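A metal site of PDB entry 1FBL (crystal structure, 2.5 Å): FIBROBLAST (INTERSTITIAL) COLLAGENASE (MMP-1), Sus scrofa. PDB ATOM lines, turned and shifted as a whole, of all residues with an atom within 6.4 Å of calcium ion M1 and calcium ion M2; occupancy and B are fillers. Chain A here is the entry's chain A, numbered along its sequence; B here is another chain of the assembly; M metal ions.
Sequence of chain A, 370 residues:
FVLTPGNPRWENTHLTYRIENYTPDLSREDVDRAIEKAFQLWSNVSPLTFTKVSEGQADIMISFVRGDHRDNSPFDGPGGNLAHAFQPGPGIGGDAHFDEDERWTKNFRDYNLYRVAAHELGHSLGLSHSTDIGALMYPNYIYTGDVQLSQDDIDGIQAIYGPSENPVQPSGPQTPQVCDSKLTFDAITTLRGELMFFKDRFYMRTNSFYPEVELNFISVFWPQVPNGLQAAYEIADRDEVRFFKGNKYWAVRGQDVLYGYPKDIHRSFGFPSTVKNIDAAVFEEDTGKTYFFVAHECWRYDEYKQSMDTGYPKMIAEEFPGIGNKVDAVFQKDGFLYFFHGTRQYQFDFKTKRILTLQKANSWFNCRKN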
ATOM      1  N   THR A  23      20.459 -13.274 -24.021  1.00  0.00           N
ATOM      2  CA  THR A  23      20.065 -14.509 -24.716  1.00  0.00           C
ATOM      3  C   THR A  23      21.072 -14.929 -25.776  1.00  0.00           C
ATOM      4  O   THR A  23      21.421 -14.112 -26.619  1.00  0.00           O
ATOM      5  CB  THR A  23      18.695 -14.334 -25.425  1.00  0.00           C
ATOM      6  OG1 THR A  23      18.323 -15.562 -26.086  1.00  0.00           O
ATOM      7  CG2 THR A  23      18.740 -13.210 -26.433  1.00  0.00           C
ATOM      8  N   PRO A  24      21.531 -16.214 -25.770  1.00  0.00           N
ATOM      9  CA  PRO A  24      22.491 -16.683 -26.792  1.00  0.00           C
ATOM     10  C   PRO A  24      21.892 -16.661 -28.209  1.00  0.00           C
ATOM     11  O   PRO A  24      22.601 -16.903 -29.168  1.00  0.00           O
ATOM     12  CB  PRO A  24      22.761 -18.129 -26.371  1.00  0.00           C
ATOM     13  CG  PRO A  24      22.445 -18.175 -24.946  1.00  0.00           C
ATOM     14  CD  PRO A  24      21.256 -17.274 -24.785  1.00  0.00           C
ATOM     15  N   ASP A  25      20.582 -16.439 -28.317  1.00  0.00           N
ATOM     16  CA  ASP A  25      19.890 -16.391 -29.609  1.00  0.00           C
ATOM     17  C   ASP A  25      20.371 -15.190 -30.457  1.00  0.00           C
ATOM     18  O   ASP A  25      20.518 -15.297 -31.657  1.00  0.00           O
ATOM     19  CB  ASP A  25      18.349 -16.327 -29.411  1.00  0.00           C
ATOM     20  CG  ASP A  25      17.776 -17.601 -28.803  1.00  0.00           C
ATOM     21  OD1 ASP A  25      18.452 -18.621 -28.798  1.00  0.00           O
ATOM     22  OD2 ASP A  25      16.646 -17.579 -28.292  1.00  0.00           O
ATOM     23  N   ARG A  66      13.428 -19.207 -17.685  1.00  0.00           N
ATOM     24  CA  ARG A  66      12.668 -20.318 -18.228  1.00  0.00           C
ATOM     25  C   ARG A  66      12.218 -21.200 -17.084  1.00  0.00           C
ATOM     26  O   ARG A  66      12.799 -21.189 -15.994  1.00  0.00           O
ATOM     27  CB  ARG A  66      13.471 -21.132 -19.230  1.00  0.00           C
ATOM     28  CG  ARG A  66      14.658 -21.815 -18.687  1.00  0.00           C
ATOM     29  CD  ARG A  66      15.251 -22.719 -19.732  1.00  0.00           C
ATOM     30  NE  ARG A  66      16.533 -22.237 -20.192  1.00  0.00           N
ATOM     31  CZ  ARG A  66      17.112 -22.631 -21.330  1.00  0.00           C
ATOM     32  NH1 ARG A  66      16.508 -23.527 -22.098  1.00  0.00           N
ATOM     33  NH2 ARG A  66      18.266 -22.104 -21.712  1.00  0.00           N
ATOM     34  N   PHE A  75       7.445 -20.243 -16.339  1.00  0.00           N
ATOM     35  CA  PHE A  75       7.188 -20.341 -17.764  1.00  0.00           C
ATOM     36  C   PHE A  75       6.824 -21.777 -18.166  1.00  0.00           C
ATOM     37  O   PHE A  75       6.820 -22.700 -17.338  1.00  0.00           O
ATOM     38  CB  PHE A  75       8.337 -19.756 -18.598  1.00  0.00           C
ATOM     39  CG  PHE A  75       8.319 -18.250 -18.670  1.00  0.00           C
ATOM     40  CD1 PHE A  75       7.155 -17.567 -18.968  1.00  0.00           C
ATOM     41  CD2 PHE A  75       9.446 -17.506 -18.361  1.00  0.00           C
ATOM     42  CE1 PHE A  75       7.129 -16.168 -18.943  1.00  0.00           C
ATOM     43  CE2 PHE A  75       9.408 -16.108 -18.343  1.00  0.00           C
ATOM     44  CZ  PHE A  75       8.273 -15.451 -18.630  1.00  0.00           C
ATOM     45  N   ASP A  76       6.537 -21.973 -19.449  1.00  0.00           N
ATOM     46  CA  ASP A  76       5.952 -23.218 -19.958  1.00  0.00           C
ATOM     47  C   ASP A  76       6.747 -23.913 -21.061  1.00  0.00           C
ATOM     48  O   ASP A  76       6.243 -24.835 -21.705  1.00  0.00           O
ATOM     49  CB  ASP A  76       4.515 -22.927 -20.463  1.00  0.00           C
ATOM     50  CG  ASP A  76       4.439 -21.823 -21.576  1.00  0.00           C
ATOM     51  OD1 ASP A  76       5.390 -21.021 -21.790  1.00  0.00           O
ATOM     52  OD2 ASP A  76       3.374 -21.749 -22.218  1.00  0.00           O
ATOM     53  N   GLY A  77       7.975 -23.467 -21.272  1.00  0.00           N
ATOM     54  CA  GLY A  77       8.754 -24.053 -22.326  1.00  0.00           C
ATOM     55  C   GLY A  77       8.503 -23.312 -23.608  1.00  0.00           C
ATOM     56  O   GLY A  77       7.970 -22.171 -23.587  1.00  0.00           O
ATOM     57  N   PRO A  78       8.892 -23.910 -24.749  1.00  0.00           N
ATOM     58  CA  PRO A  78       8.752 -23.368 -26.101  1.00  0.00           C
ATOM     59  C   PRO A  78       7.300 -23.011 -26.439  1.00  0.00           C
ATOM     60  O   PRO A  78       6.366 -23.813 -26.195  1.00  0.00           O
ATOM     61  CB  PRO A  78       9.271 -24.511 -26.974  1.00  0.00           C
ATOM     62  CG  PRO A  78      10.179 -25.281 -26.084  1.00  0.00           C
ATOM     63  CD  PRO A  78       9.439 -25.276 -24.799  1.00  0.00           C
ATOM     64  N   GLY A  79       7.128 -21.803 -26.996  1.00  0.00           N
ATOM     65  CA  GLY A  79       5.829 -21.278 -27.365  1.00  0.00           C
ATOM     66  C   GLY A  79       4.919 -20.875 -26.227  1.00  0.00           C
ATOM     67  O   GLY A  79       5.354 -20.749 -25.060  1.00  0.00           O
ATOM     68  N   GLY A  80       3.663 -20.647 -26.575  1.00  0.00           N
ATOM     69  CA  GLY A  80       2.644 -20.286 -25.628  1.00  0.00           C
ATOM     70  C   GLY A  80       3.068 -19.003 -24.969  1.00  0.00           C
ATOM     71  O   GLY A  80       3.337 -18.047 -25.667  1.00  0.00           O
ATOM     72  N   ASN A  81       3.165 -19.036 -23.635  1.00  0.00           N
ATOM     73  CA  ASN A  81       3.675 -17.963 -22.781  1.00  0.00           C
ATOM     74  C   ASN A  81       5.127 -17.616 -23.198  1.00  0.00           C
ATOM     75  O   ASN A  81       6.047 -18.514 -23.163  1.00  0.00           O
ATOM     76  CB  ASN A  81       3.643 -18.459 -21.339  1.00  0.00           C
ATOM     77  CG  ASN A  81       3.653 -17.355 -20.319  1.00  0.00           C
ATOM     78  OD1 ASN A  81       3.669 -16.157 -20.643  1.00  0.00           O
ATOM     79  ND2 ASN A  81       3.590 -17.742 -19.057  1.00  0.00           N
ATOM     80  N   LEU A  82       5.287 -16.354 -23.636  1.00  0.00           N
ATOM     81  CA  LEU A  82       6.554 -15.799 -24.139  1.00  0.00           C
ATOM     82  C   LEU A  82       7.260 -14.968 -23.086  1.00  0.00           C
ATOM     83  O   LEU A  82       8.466 -15.105 -22.907  1.00  0.00           O
ATOM     84  CB  LEU A  82       6.316 -14.862 -25.348  1.00  0.00           C
ATOM     85  CG  LEU A  82       5.358 -15.047 -26.548  1.00  0.00           C
ATOM     86  CD1 LEU A  82       5.725 -14.066 -27.598  1.00  0.00           C
ATOM     87  CD2 LEU A  82       5.469 -16.431 -27.109  1.00  0.00           C
ATOM     88  N   ALA A  83       6.528 -14.098 -22.401  1.00  0.00           N
ATOM     89  CA  ALA A  83       7.128 -13.209 -21.413  1.00  0.00           C
ATOM     90  C   ALA A  83       6.106 -12.650 -20.456  1.00  0.00           C
ATOM     91  O   ALA A  83       4.910 -12.845 -20.657  1.00  0.00           O
ATOM     92  CB  ALA A  83       7.840 -12.072 -22.126  1.00  0.00           C
ATOM     93  N   ASP A  99      10.889 -15.652 -21.505  1.00  0.00           N
ATOM     94  CA  ASP A  99      11.111 -17.128 -21.567  1.00  0.00           C
ATOM     95  C   ASP A  99      12.208 -17.598 -22.579  1.00  0.00           C
ATOM     96  O   ASP A  99      12.003 -17.570 -23.786  1.00  0.00           O
ATOM     97  CB  ASP A  99       9.773 -17.803 -21.857  1.00  0.00           C
ATOM     98  CG  ASP A  99       9.833 -19.300 -21.842  1.00  0.00           C
ATOM     99  OD1 ASP A  99      10.855 -19.883 -21.444  1.00  0.00           O
ATOM    100  OD2 ASP A  99       8.824 -19.920 -22.236  1.00  0.00           O
ATOM    101  N   GLU A 100      13.329 -18.128 -22.084  1.00  0.00           N
ATOM    102  CA  GLU A 100      14.505 -18.438 -22.907  1.00  0.00           C
ATOM    103  C   GLU A 100      14.345 -19.634 -23.831  1.00  0.00           C
ATOM    104  O   GLU A 100      15.130 -19.826 -24.793  1.00  0.00           O
ATOM    105  CB  GLU A 100      15.745 -18.624 -22.027  1.00  0.00           C
ATOM    106  CG  GLU A 100      17.018 -18.844 -22.771  1.00  0.00           C
ATOM    107  CD  GLU A 100      17.367 -17.682 -23.664  1.00  0.00           C
ATOM    108  OE1 GLU A 100      17.812 -16.675 -23.105  1.00  0.00           O
ATOM    109  OE2 GLU A 100      17.185 -17.770 -24.918  1.00  0.00           O
ATOM    110  N   ASP A 101      13.301 -20.424 -23.526  1.00  0.00           N
ATOM    111  CA  ASP A 101      12.871 -21.562 -24.339  1.00  0.00           C
ATOM    112  C   ASP A 101      12.317 -21.071 -25.659  1.00  0.00           C
ATOM    113  O   ASP A 101      12.023 -21.886 -26.526  1.00  0.00           O
ATOM    114  CB  ASP A 101      11.777 -22.375 -23.649  1.00  0.00           C
ATOM    115  CG  ASP A 101      12.291 -23.277 -22.527  1.00  0.00           C
ATOM    116  OD1 ASP A 101      13.413 -23.854 -22.615  1.00  0.00           O
ATOM    117  OD2 ASP A 101      11.529 -23.433 -21.549  1.00  0.00           O
ATOM    118  N   GLU A 102      12.072 -19.750 -25.771  1.00  0.00           N
ATOM    119  CA  GLU A 102      11.687 -19.116 -27.039  1.00  0.00           C
ATOM    120  C   GLU A 102      12.914 -18.770 -27.919  1.00  0.00           C
ATOM    121  O   GLU A 102      14.015 -18.390 -27.419  1.00  0.00           O
ATOM    122  CB  GLU A 102      10.860 -17.834 -26.820  1.00  0.00           C
ATOM    123  CG  GLU A 102       9.652 -17.929 -25.935  1.00  0.00           C
ATOM    124  CD  GLU A 102       8.777 -19.109 -26.263  1.00  0.00           C
ATOM    125  OE1 GLU A 102       8.919 -19.700 -27.364  1.00  0.00           O
ATOM    126  OE2 GLU A 102       7.963 -19.491 -25.402  1.00  0.00           O
ATOM    127  N   ARG A 103      12.772 -18.971 -29.223  1.00  0.00           N
ATOM    128  CA  ARG A 103      13.808 -18.554 -30.174  1.00  0.00           C
ATOM    129  C   ARG A 103      13.647 -17.034 -30.357  1.00  0.00           C
ATOM    130  O   ARG A 103      12.690 -16.571 -31.004  1.00  0.00           O
ATOM    131  CB  ARG A 103      13.622 -19.285 -31.503  1.00  0.00           C
ATOM    132  CG  ARG A 103      14.886 -19.457 -32.335  1.00  0.00           C
ATOM    133  CD  ARG A 103      15.498 -18.145 -32.720  1.00  0.00           C
ATOM    134  NE  ARG A 103      16.506 -18.323 -33.752  1.00  0.00           N
ATOM    135  CZ  ARG A 103      17.799 -18.506 -33.503  1.00  0.00           C
ATOM    136  NH1 ARG A 103      18.267 -18.466 -32.263  1.00  0.00           N
ATOM    137  NH2 ARG A 103      18.635 -18.826 -34.500  1.00  0.00           N
ATOM    138  N   TRP A 104      14.533 -16.263 -29.748  1.00  0.00           N
ATOM    139  CA  TRP A 104      14.427 -14.821 -29.858  1.00  0.00           C
ATOM    140  C   TRP A 104      14.956 -14.325 -31.186  1.00  0.00           C
ATOM    141  O   TRP A 104      16.111 -14.569 -31.522  1.00  0.00           O
ATOM    142  CB  TRP A 104      15.121 -14.172 -28.653  1.00  0.00           C
ATOM    143  CG  TRP A 104      14.312 -14.417 -27.351  1.00  0.00           C
ATOM    144  CD1 TRP A 104      14.699 -15.159 -26.283  1.00  0.00           C
ATOM    145  CD2 TRP A 104      12.937 -14.033 -27.104  1.00  0.00           C
ATOM    146  NE1 TRP A 104      13.665 -15.280 -25.397  1.00  0.00           N
ATOM    147  CE2 TRP A 104      12.576 -14.605 -25.882  1.00  0.00           C
ATOM    148  CE3 TRP A 104      12.002 -13.265 -27.807  1.00  0.00           C
ATOM    149  CZ2 TRP A 104      11.300 -14.437 -25.335  1.00  0.00           C
ATOM    150  CZ3 TRP A 104      10.758 -13.099 -27.277  1.00  0.00           C
ATOM    151  CH2 TRP A 104      10.412 -13.684 -26.050  1.00  0.00           C
ATOM    152  N   ASN B 140       1.268 -26.345 -26.868  1.00  0.00           N
ATOM    153  CA  ASN B 140       1.347 -25.125 -27.650  1.00  0.00           C
ATOM    154  C   ASN B 140       1.499 -25.362 -29.151  1.00  0.00           C
ATOM    155  O   ASN B 140       2.122 -26.339 -29.578  1.00  0.00           O
ATOM    156  CB  ASN B 140       2.533 -24.277 -27.201  1.00  0.00           C
ATOM    157  CG  ASN B 140       2.496 -23.913 -25.731  1.00  0.00           C
ATOM    158  OD1 ASN B 140       3.557 -23.678 -25.144  1.00  0.00           O
ATOM    159  ND2 ASN B 140       1.303 -23.789 -25.137  1.00  0.00           N
ATOM    160  N   ARG B 205      21.182 -28.396 -27.952  1.00  0.00           N
ATOM    161  CA  ARG B 205      22.094 -27.302 -27.672  1.00  0.00           C
ATOM    162  C   ARG B 205      22.633 -27.446 -26.242  1.00  0.00           C
ATOM    163  O   ARG B 205      21.915 -27.911 -25.356  1.00  0.00           O
ATOM    164  CB  ARG B 205      21.313 -25.997 -27.829  1.00  0.00           C
ATOM    165  CG  ARG B 205      22.063 -24.705 -27.682  1.00  0.00           C
ATOM    166  CD  ARG B 205      21.072 -23.635 -28.054  1.00  0.00           C
ATOM    167  NE  ARG B 205      21.593 -22.273 -28.030  1.00  0.00           N
ATOM    168  CZ  ARG B 205      20.881 -21.207 -28.359  1.00  0.00           C
ATOM    169  NH1 ARG B 205      19.639 -21.330 -28.752  1.00  0.00           N
ATOM    170  NH2 ARG B 205      21.389 -19.999 -28.270  1.00  0.00           N
ATOM    171  N   TYR B 210      24.972 -24.301 -19.597  1.00  0.00           N
ATOM    172  CA  TYR B 210      23.652 -24.939 -19.540  1.00  0.00           C
ATOM    173  C   TYR B 210      23.341 -26.022 -18.475  1.00  0.00           C
ATOM    174  O   TYR B 210      23.942 -27.108 -18.468  1.00  0.00           O
ATOM    175  CB  TYR B 210      23.316 -25.540 -20.904  1.00  0.00           C
ATOM    176  CG  TYR B 210      22.800 -24.546 -21.904  1.00  0.00           C
ATOM    177  CD1 TYR B 210      23.533 -23.404 -22.206  1.00  0.00           C
ATOM    178  CD2 TYR B 210      21.583 -24.764 -22.563  1.00  0.00           C
ATOM    179  CE1 TYR B 210      23.092 -22.499 -23.136  1.00  0.00           C
ATOM    180  CE2 TYR B 210      21.122 -23.873 -23.516  1.00  0.00           C
ATOM    181  CZ  TYR B 210      21.877 -22.731 -23.796  1.00  0.00           C
ATOM    182  OH  TYR B 210      21.437 -21.799 -24.701  1.00  0.00           O
ATOM    183  N   GLU B 214      19.156 -28.360 -24.336  1.00  0.00           N
ATOM    184  CA  GLU B 214      17.922 -27.792 -24.847  1.00  0.00           C
ATOM    185  C   GLU B 214      17.529 -28.563 -26.101  1.00  0.00           C
ATOM    186  O   GLU B 214      18.242 -28.546 -27.107  1.00  0.00           O
ATOM    187  CB  GLU B 214      18.117 -26.311 -25.177  1.00  0.00           C
ATOM    188  CG  GLU B 214      17.090 -25.790 -26.173  1.00  0.00           C
ATOM    189  CD  GLU B 214      17.332 -24.344 -26.562  1.00  0.00           C
ATOM    190  OE1 GLU B 214      17.359 -23.473 -25.672  1.00  0.00           O
ATOM    191  OE2 GLU B 214      17.511 -24.069 -27.771  1.00  0.00           O
ATOM    192  N   PHE B 221      14.696 -23.099 -35.032  1.00  0.00           N
ATOM    193  CA  PHE B 221      15.945 -22.384 -34.857  1.00  0.00           C
ATOM    194  C   PHE B 221      16.324 -21.650 -36.141  1.00  0.00           C
ATOM    195  O   PHE B 221      16.591 -20.464 -36.102  1.00  0.00           O
ATOM    196  CB  PHE B 221      17.059 -23.354 -34.494  1.00  0.00           C
ATOM    197  CG  PHE B 221      18.053 -22.793 -33.557  1.00  0.00           C
ATOM    198  CD1 PHE B 221      17.659 -22.417 -32.277  1.00  0.00           C
ATOM    199  CD2 PHE B 221      19.341 -22.476 -33.988  1.00  0.00           C
ATOM    200  CE1 PHE B 221      18.515 -21.728 -31.447  1.00  0.00           C
ATOM    201  CE2 PHE B 221      20.222 -21.782 -33.179  1.00  0.00           C
ATOM    202  CZ  PHE B 221      19.816 -21.408 -31.905  1.00  0.00           C
HETATM  203 CA    CA M   1      16.335 -19.146 -26.458  1.00  0.00          CA
HETATM  204 CA    CA M   2       6.905 -20.260 -23.554  1.00  0.00          CA
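OD1 of Asp 25 is in salt-bridge range of NH1 of Arg 103. N of Asp 25 lies close to OG1 of Thr 23 (3.3 Å). OD1 of Asp 99 lies close to N of Asp 101. The backbone carbonyl oxygen (O) of Leu 82 is in hydrogen-bond range of the backbone NH (N) of Asp 99 (2.9 Å). The backbone carbonyl oxygen (O) of Asp 99 lies within hydrogen-bond range of the indole nitrogen (NE1) of Trp 104, 3.3 Å away. The side-chain carboxylate (OD1) of Asp 25 is in salt-bridge range of the guanidinium group (NH1) of Arg 205 of chain B. The side-chain carboxylate of Asp 25 lies close to the backbone NH of Trp 104, at 2.9 Å. The backbone carbonyl oxygen of Gly 79 lies close to the side-chain amide oxygen of Asn 140 of chain B.
Three residues have an atom within 4 Å of calcium ion M1: Asp 25, Glu 100 and Glu 102. The nearest printed residue that does not touch calcium ion M1 is Thr 23 (4.1 Å).
Of the 24 residues printed, 6 come within 4 Å of calcium ion M2.
Calcium ion M1 is bound by O of Glu 100 (2.2 Å), OE2 of Glu 100 (2.2 Å), OD2 of Asp 25 (2.4 Å) and O of Glu 102 (2.6 Å). Calcium ion M1 has four donor atoms within binding distance.
Calcium ion M2 is bound by the backbone carbonyl oxygen (O) of Asn 81 (2.0 Å), the backbone carbonyl oxygen (O) of Gly 77 (2.2 Å), the backbone carbonyl oxygen (O) of Gly 79 (2.2 Å), the side-chain carboxylate (OE2) of Glu 102 (2.3 Å), the side-chain carboxylate (OD2) of Asp 99 (2.4 Å) and the side-chain carboxylate (OD1) of Asp 76 (2.4 Å). Calcium ion M2 has six donor atoms within binding distance.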
